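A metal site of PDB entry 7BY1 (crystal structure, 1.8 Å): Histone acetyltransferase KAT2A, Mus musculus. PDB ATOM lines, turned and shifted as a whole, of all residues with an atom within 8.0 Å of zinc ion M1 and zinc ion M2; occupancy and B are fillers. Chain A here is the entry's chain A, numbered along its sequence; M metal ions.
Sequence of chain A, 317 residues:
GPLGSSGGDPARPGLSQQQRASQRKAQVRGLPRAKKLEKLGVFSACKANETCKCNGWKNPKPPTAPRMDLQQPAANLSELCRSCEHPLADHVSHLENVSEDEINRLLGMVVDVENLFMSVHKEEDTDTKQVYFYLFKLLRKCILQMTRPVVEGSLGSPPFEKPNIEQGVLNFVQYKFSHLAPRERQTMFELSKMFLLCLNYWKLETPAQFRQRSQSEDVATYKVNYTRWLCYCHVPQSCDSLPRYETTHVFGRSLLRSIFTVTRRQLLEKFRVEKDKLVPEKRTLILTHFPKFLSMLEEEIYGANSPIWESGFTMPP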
ATOM      1  N   GLY A  41      18.012  13.420 -20.580  1.00  0.00           N
ATOM      2  CA  GLY A  41      17.628  14.725 -20.055  1.00  0.00           C
ATOM      3  C   GLY A  41      18.372  15.864 -20.722  1.00  0.00           C
ATOM      4  O   GLY A  41      17.816  16.944 -20.969  1.00  0.00           O
ATOM      5  N   SER A  44      16.178  16.816 -23.657  1.00  0.00           N
ATOM      6  CA  SER A  44      14.726  16.855 -23.393  1.00  0.00           C
ATOM      7  C   SER A  44      14.225  18.216 -22.875  1.00  0.00           C
ATOM      8  O   SER A  44      14.900  18.864 -22.105  1.00  0.00           O
ATOM      9  CB  SER A  44      14.329  15.765 -22.413  1.00  0.00           C
ATOM     10  OG  SER A  44      14.678  14.459 -22.860  1.00  0.00           O
ATOM     11  N   ALA A  45      12.998  18.567 -23.267  1.00  0.00           N
ATOM     12  CA  ALA A  45      12.372  19.867 -22.937  1.00  0.00           C
ATOM     13  C   ALA A  45      12.003  19.945 -21.487  1.00  0.00           C
ATOM     14  O   ALA A  45      11.588  18.967 -20.863  1.00  0.00           O
ATOM     15  CB  ALA A  45      11.129  20.091 -23.782  1.00  0.00           C
ATOM     16  N   CYS A  46      12.156  21.125 -20.915  1.00  0.00           N
ATOM     17  CA  CYS A  46      11.736  21.336 -19.524  1.00  0.00           C
ATOM     18  C   CYS A  46      10.223  21.526 -19.494  1.00  0.00           C
ATOM     19  O   CYS A  46       9.705  22.245 -20.316  1.00  0.00           O
ATOM     20  CB  CYS A  46      12.451  22.535 -18.918  1.00  0.00           C
ATOM     21  SG  CYS A  46      12.062  22.717 -17.147  1.00  0.00           S
ATOM     22  N   LYS A  47       9.550  20.879 -18.546  1.00  0.00           N
ATOM     23  CA  LYS A  47       8.113  21.119 -18.341  1.00  0.00           C
ATOM     24  C   LYS A  47       7.894  21.514 -16.888  1.00  0.00           C
ATOM     25  O   LYS A  47       6.869  21.162 -16.309  1.00  0.00           O
ATOM     26  CB  LYS A  47       7.296  19.862 -18.679  1.00  0.00           C
ATOM     27  CG  LYS A  47       7.635  19.192 -20.021  1.00  0.00           C
ATOM     28  CD  LYS A  47       7.681  17.668 -19.801  1.00  0.00           C
ATOM     29  CE  LYS A  47       8.419  16.996 -20.901  1.00  0.00           C
ATOM     30  NZ  LYS A  47       9.893  16.999 -20.803  1.00  0.00           N
ATOM     31  N   ALA A  48       8.857  22.182 -16.263  1.00  0.00           N
ATOM     32  CA  ALA A  48       8.639  22.695 -14.883  1.00  0.00           C
ATOM     33  C   ALA A  48       7.377  23.579 -14.767  1.00  0.00           C
ATOM     34  O   ALA A  48       6.708  23.559 -13.721  1.00  0.00           O
ATOM     35  CB  ALA A  48       9.832  23.487 -14.429  1.00  0.00           C
ATOM     36  N   ASN A  49       7.087  24.354 -15.815  1.00  0.00           N
ATOM     37  CA  ASN A  49       5.933  25.257 -15.831  1.00  0.00           C
ATOM     38  C   ASN A  49       5.602  25.541 -17.277  1.00  0.00           C
ATOM     39  O   ASN A  49       6.359  25.138 -18.170  1.00  0.00           O
ATOM     40  CB  ASN A  49       6.221  26.572 -15.057  1.00  0.00           C
ATOM     41  CG  ASN A  49       7.451  27.328 -15.566  1.00  0.00           C
ATOM     42  OD1 ASN A  49       7.508  27.717 -16.731  1.00  0.00           O
ATOM     43  ND2 ASN A  49       8.407  27.567 -14.696  1.00  0.00           N
ATOM     44  N   THR A  51       5.826  28.268 -18.977  1.00  0.00           N
ATOM     45  CA  THR A  51       6.644  29.305 -19.647  1.00  0.00           C
ATOM     46  C   THR A  51       8.134  28.933 -19.954  1.00  0.00           C
ATOM     47  O   THR A  51       8.742  29.538 -20.824  1.00  0.00           O
ATOM     48  CB  THR A  51       6.637  30.641 -18.855  1.00  0.00           C
ATOM     49  OG1 THR A  51       7.336  30.479 -17.616  1.00  0.00           O
ATOM     50  CG2 THR A  51       5.192  31.123 -18.564  1.00  0.00           C
ATOM     51  N   CYS A  52       8.705  27.973 -19.213  1.00  0.00           N
ATOM     52  CA  CYS A  52      10.131  27.615 -19.427  1.00  0.00           C
ATOM     53  C   CYS A  52      10.294  27.028 -20.815  1.00  0.00           C
ATOM     54  O   CYS A  52       9.602  26.099 -21.174  1.00  0.00           O
ATOM     55  CB  CYS A  52      10.639  26.647 -18.358  1.00  0.00           C
ATOM     56  SG  CYS A  52      12.426  26.297 -18.486  1.00  0.00           S
ATOM     57  N   LYS A  53      11.191  27.609 -21.602  1.00  0.00           N
ATOM     58  CA  LYS A  53      11.448  27.133 -22.973  1.00  0.00           C
ATOM     59  C   LYS A  53      12.773  26.328 -23.111  1.00  0.00           C
ATOM     60  O   LYS A  53      13.251  26.137 -24.225  1.00  0.00           O
ATOM     61  CB  LYS A  53      11.573  28.347 -23.902  1.00  0.00           C
ATOM     62  CG  LYS A  53      10.368  29.304 -24.000  1.00  0.00           C
ATOM     63  CD  LYS A  53      10.823  30.720 -24.402  1.00  0.00           C
ATOM     64  CE  LYS A  53      12.092  30.759 -25.288  1.00  0.00           C
ATOM     65  NZ  LYS A  53      12.544  32.120 -25.694  1.00  0.00           N
ATOM     66  N   CYS A  54      13.380  25.903 -22.016  1.00  0.00           N
ATOM     67  CA  CYS A  54      14.643  25.153 -22.095  1.00  0.00           C
ATOM     68  C   CYS A  54      14.458  23.845 -22.860  1.00  0.00           C
ATOM     69  O   CYS A  54      13.436  23.180 -22.703  1.00  0.00           O
ATOM     70  CB  CYS A  54      15.096  24.807 -20.691  1.00  0.00           C
ATOM     71  SG  CYS A  54      16.637  23.847 -20.529  1.00  0.00           S
ATOM     72  N   ASN A  55      15.434  23.516 -23.708  1.00  0.00           N
ATOM     73  CA  ASN A  55      15.356  22.327 -24.584  1.00  0.00           C
ATOM     74  C   ASN A  55      16.345  21.238 -24.131  1.00  0.00           C
ATOM     75  O   ASN A  55      16.618  20.287 -24.876  1.00  0.00           O
ATOM     76  CB  ASN A  55      15.708  22.702 -26.042  1.00  0.00           C
ATOM     77  CG  ASN A  55      14.688  23.618 -26.693  1.00  0.00           C
ATOM     78  OD1 ASN A  55      15.066  24.459 -27.518  1.00  0.00           O
ATOM     79  ND2 ASN A  55      13.390  23.464 -26.353  1.00  0.00           N
ATOM     80  N   GLY A  56      16.977  21.405 -22.963  1.00  0.00           N
ATOM     81  CA  GLY A  56      17.906  20.379 -22.503  1.00  0.00           C
ATOM     82  C   GLY A  56      18.487  20.649 -21.118  1.00  0.00           C
ATOM     83  O   GLY A  56      18.958  21.757 -20.880  1.00  0.00           O
ATOM     84  N   TRP A  57      18.460  19.653 -20.221  1.00  0.00           N
ATOM     85  CA  TRP A  57      19.069  19.773 -18.899  1.00  0.00           C
ATOM     86  C   TRP A  57      20.566  19.854 -19.009  1.00  0.00           C
ATOM     87  O   TRP A  57      21.190  18.934 -19.539  1.00  0.00           O
ATOM     88  CB  TRP A  57      18.731  18.607 -17.966  1.00  0.00           C
ATOM     89  CG  TRP A  57      19.344  18.640 -16.574  1.00  0.00           C
ATOM     90  CD1 TRP A  57      18.867  19.296 -15.476  1.00  0.00           C
ATOM     91  CD2 TRP A  57      20.447  17.884 -16.123  1.00  0.00           C
ATOM     92  NE1 TRP A  57      19.655  19.061 -14.393  1.00  0.00           N
ATOM     93  CE2 TRP A  57      20.629  18.181 -14.741  1.00  0.00           C
ATOM     94  CE3 TRP A  57      21.330  17.012 -16.733  1.00  0.00           C
ATOM     95  CZ2 TRP A  57      21.640  17.653 -13.989  1.00  0.00           C
ATOM     96  CZ3 TRP A  57      22.330  16.433 -15.997  1.00  0.00           C
ATOM     97  CH2 TRP A  57      22.479  16.735 -14.609  1.00  0.00           C
ATOM     98  N   LYS A  58      21.124  20.927 -18.426  1.00  0.00           N
ATOM     99  CA  LYS A  58      22.608  21.101 -18.375  1.00  0.00           C
ATOM    100  C   LYS A  58      23.160  20.883 -17.004  1.00  0.00           C
ATOM    101  O   LYS A  58      22.839  21.600 -16.079  1.00  0.00           O
ATOM    102  CB  LYS A  58      22.985  22.503 -18.894  1.00  0.00           C
ATOM    103  CG  LYS A  58      22.564  22.787 -20.329  1.00  0.00           C
ATOM    104  CD  LYS A  58      23.450  22.016 -21.313  1.00  0.00           C
ATOM    105  CE  LYS A  58      22.847  21.978 -22.714  1.00  0.00           C
ATOM    106  NZ  LYS A  58      22.982  23.289 -23.399  1.00  0.00           N
ATOM    107  N   LEU A  80      19.765  20.989 -10.396  1.00  0.00           N
ATOM    108  CA  LEU A  80      19.137  22.089 -11.138  1.00  0.00           C
ATOM    109  C   LEU A  80      19.892  22.399 -12.437  1.00  0.00           C
ATOM    110  O   LEU A  80      21.081  22.603 -12.409  1.00  0.00           O
ATOM    111  CB  LEU A  80      19.124  23.343 -10.267  1.00  0.00           C
ATOM    112  CG  LEU A  80      18.339  23.259  -8.943  1.00  0.00           C
ATOM    113  CD1 LEU A  80      18.344  24.619  -8.232  1.00  0.00           C
ATOM    114  CD2 LEU A  80      16.903  22.823  -9.104  1.00  0.00           C
ATOM    115  N   CYS A  81      19.162  22.494 -13.530  1.00  0.00           N
ATOM    116  CA  CYS A  81      19.678  22.820 -14.825  1.00  0.00           C
ATOM    117  C   CYS A  81      20.478  24.160 -14.780  1.00  0.00           C
ATOM    118  O   CYS A  81      19.939  25.169 -14.311  1.00  0.00           O
ATOM    119  CB  CYS A  81      18.515  22.989 -15.777  1.00  0.00           C
ATOM    120  SG  CYS A  81      18.849  23.301 -17.543  1.00  0.00           S
ATOM    121  N   ARG A  82      21.730  24.150 -15.259  1.00  0.00           N
ATOM    122  CA  ARG A  82      22.474  25.437 -15.457  1.00  0.00           C
ATOM    123  C   ARG A  82      21.685  26.502 -16.210  1.00  0.00           C
ATOM    124  O   ARG A  82      21.822  27.697 -15.934  1.00  0.00           O
ATOM    125  CB  ARG A  82      23.724  25.265 -16.293  1.00  0.00           C
ATOM    126  CG  ARG A  82      24.852  24.668 -15.573  1.00  0.00           C
ATOM    127  CD  ARG A  82      26.110  24.827 -16.382  1.00  0.00           C
ATOM    128  NE  ARG A  82      27.043  23.819 -15.963  1.00  0.00           N
ATOM    129  CZ  ARG A  82      28.351  23.795 -16.192  1.00  0.00           C
ATOM    130  NH1 ARG A  82      28.930  24.782 -16.841  1.00  0.00           N
ATOM    131  NH2 ARG A  82      29.059  22.762 -15.773  1.00  0.00           N
ATOM    132  N   SER A  83      20.937  26.109 -17.246  1.00  0.00           N
ATOM    133  CA  SER A  83      20.248  27.100 -18.073  1.00  0.00           C
ATOM    134  C   SER A  83      19.006  27.669 -17.448  1.00  0.00           C
ATOM    135  O   SER A  83      18.760  28.884 -17.536  1.00  0.00           O
ATOM    136  CB  SER A  83      19.827  26.498 -19.428  1.00  0.00           C
ATOM    137  OG  SER A  83      20.910  25.850 -20.061  1.00  0.00           O
ATOM    138  N   CYS A  84      18.173  26.801 -16.887  1.00  0.00           N
ATOM    139  CA  CYS A  84      16.811  27.202 -16.520  1.00  0.00           C
ATOM    140  C   CYS A  84      16.559  27.048 -15.024  1.00  0.00           C
ATOM    141  O   CYS A  84      15.489  27.435 -14.555  1.00  0.00           O
ATOM    142  CB  CYS A  84      15.783  26.398 -17.370  1.00  0.00           C
ATOM    143  SG  CYS A  84      15.369  24.714 -16.826  1.00  0.00           S
ATOM    144  N   GLU A  85      17.522  26.486 -14.284  1.00  0.00           N
ATOM    145  CA  GLU A  85      17.434  26.262 -12.836  1.00  0.00           C
ATOM    146  C   GLU A  85      16.229  25.415 -12.335  1.00  0.00           C
ATOM    147  O   GLU A  85      15.793  25.543 -11.180  1.00  0.00           O
ATOM    148  CB  GLU A  85      17.562  27.630 -12.093  1.00  0.00           C
ATOM    149  CG  GLU A  85      18.816  28.389 -12.529  1.00  0.00           C
ATOM    150  CD  GLU A  85      20.082  28.085 -11.724  1.00  0.00           C
ATOM    151  OE1 GLU A  85      20.181  27.028 -11.041  1.00  0.00           O
ATOM    152  OE2 GLU A  85      20.992  28.978 -11.744  1.00  0.00           O
ATOM    153  N   HIS A  86      15.743  24.503 -13.190  1.00  0.00           N
ATOM    154  CA  HIS A  86      14.710  23.577 -12.826  1.00  0.00           C
ATOM    155  C   HIS A  86      15.352  22.202 -12.753  1.00  0.00           C
ATOM    156  O   HIS A  86      16.347  21.917 -13.442  1.00  0.00           O
ATOM    157  CB  HIS A  86      13.521  23.647 -13.771  1.00  0.00           C
ATOM    158  CG  HIS A  86      12.843  24.987 -13.784  1.00  0.00           C
ATOM    159  ND1 HIS A  86      12.575  25.678 -14.952  1.00  0.00           N
ATOM    160  CD2 HIS A  86      12.416  25.793 -12.768  1.00  0.00           C
ATOM    161  CE1 HIS A  86      11.949  26.819 -14.677  1.00  0.00           C
ATOM    162  NE2 HIS A  86      11.866  26.919 -13.352  1.00  0.00           N
ATOM    163  N   PRO A  87      14.819  21.326 -11.909  1.00  0.00           N
ATOM    164  CA  PRO A  87      15.486  20.046 -11.701  1.00  0.00           C
ATOM    165  C   PRO A  87      15.496  19.171 -12.995  1.00  0.00           C
ATOM    166  O   PRO A  87      14.620  19.360 -13.860  1.00  0.00           O
ATOM    167  CB  PRO A  87      14.585  19.347 -10.670  1.00  0.00           C
ATOM    168  CG  PRO A  87      13.923  20.441  -9.929  1.00  0.00           C
ATOM    169  CD  PRO A  87      13.756  21.572 -10.889  1.00  0.00           C
ATOM    170  N   LEU A  88      16.446  18.262 -13.049  1.00  0.00           N
ATOM    171  CA  LEU A  88      16.486  17.176 -14.086  1.00  0.00           C
ATOM    172  C   LEU A  88      15.100  16.498 -14.156  1.00  0.00           C
ATOM    173  O   LEU A  88      14.582  16.312 -15.250  1.00  0.00           O
ATOM    174  CB  LEU A  88      17.604  16.194 -13.782  1.00  0.00           C
ATOM    175  CG  LEU A  88      17.700  14.882 -14.568  1.00  0.00           C
ATOM    176  CD1 LEU A  88      17.795  15.157 -16.051  1.00  0.00           C
ATOM    177  CD2 LEU A  88      18.857  14.070 -14.056  1.00  0.00           C
ATOM    178  N   ASP A  90      12.183  17.609 -13.987  1.00  0.00           N
ATOM    179  CA  ASP A  90      11.217  18.300 -14.812  1.00  0.00           C
ATOM    180  C   ASP A  90      11.522  18.205 -16.337  1.00  0.00           C
ATOM    181  O   ASP A  90      10.694  18.586 -17.136  1.00  0.00           O
ATOM    182  CB  ASP A  90      11.090  19.750 -14.427  1.00  0.00           C
ATOM    183  CG  ASP A  90      10.640  19.969 -12.959  1.00  0.00           C
ATOM    184  OD1 ASP A  90      10.000  19.121 -12.351  1.00  0.00           O
ATOM    185  OD2 ASP A  90      10.937  21.054 -12.454  1.00  0.00           O
ATOM    186  N   HIS A  91      12.755  17.823 -16.679  1.00  0.00           N
ATOM    187  CA  HIS A  91      13.140  17.650 -18.088  1.00  0.00           C
ATOM    188  C   HIS A  91      12.861  16.192 -18.553  1.00  0.00           C
ATOM    189  O   HIS A  91      12.668  15.999 -19.755  1.00  0.00           O
ATOM    190  CB  HIS A  91      14.631  17.952 -18.281  1.00  0.00           C
ATOM    191  CG  HIS A  91      15.015  19.365 -17.912  1.00  0.00           C
ATOM    192  ND1 HIS A  91      15.048  19.819 -16.601  1.00  0.00           N
ATOM    193  CD2 HIS A  91      15.470  20.383 -18.677  1.00  0.00           C
ATOM    194  CE1 HIS A  91      15.483  21.067 -16.584  1.00  0.00           C
ATOM    195  NE2 HIS A  91      15.742  21.431 -17.827  1.00  0.00           N
HETATM  196 ZN    ZN M   1      13.002  24.775 -16.949  1.00  0.00          ZN
HETATM  197 ZN    ZN M   2      16.713  23.325 -18.357  1.00  0.00          ZN
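O of Cys 54 sits at hydrogen-bond distance from N of Cys 46 (3.0 Å). N of Cys 54 lies close to SG of Cys 52, at 3.7 Å. The backbone carbonyl oxygen (O) of His 91 sits at hydrogen-bond distance from the side-chain amino group (NZ) of Lys 47. The side-chain sulfur of Cys 54 sits close to the backbone carbonyl oxygen of Gly 56 (3.1 Å). N of Ser 83 lies close to SG of Cys 81, 3.5 Å away. N of Cys 52 sits at hydrogen-bond distance from OD1 of Asn 49 (2.8 Å). The backbone NH of Gly 56 sits close to the backbone carbonyl oxygen of Ser 44, 3.4 Å away. The backbone carbonyl oxygen (O) of Pro 87 lies within hydrogen-bond range of a ring nitrogen (ND1) of His 91.
The nearest printed residue that does not touch zinc ion M1 is Ala 48 (4.2 Å).
O of Gly 56 touches zinc ion M2, 3.7 Å away. Of the 26 residues printed, 5 come within 4 Å of zinc ion M2. The nearest printed residue that does not touch zinc ion M2 is Trp 57 (4.3 Å).
Zinc ion M1 is bound by a ring nitrogen (ND1) of His 86 (2.2 Å), the side-chain sulfur of Cys 52 (2.2 Å), the side-chain sulfur of Cys 46 (2.3 Å) and the side-chain sulfur of Cys 84 (2.4 Å).
Zinc ion M2 is bound by NE2 of His 91 (2.2 Å), SG of Cys 54 (2.2 Å), SG of Cys 81 (2.3 Å) and SG of Cys 84 (2.5 Å). Zinc ion M2 has four donor atoms within binding distance.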
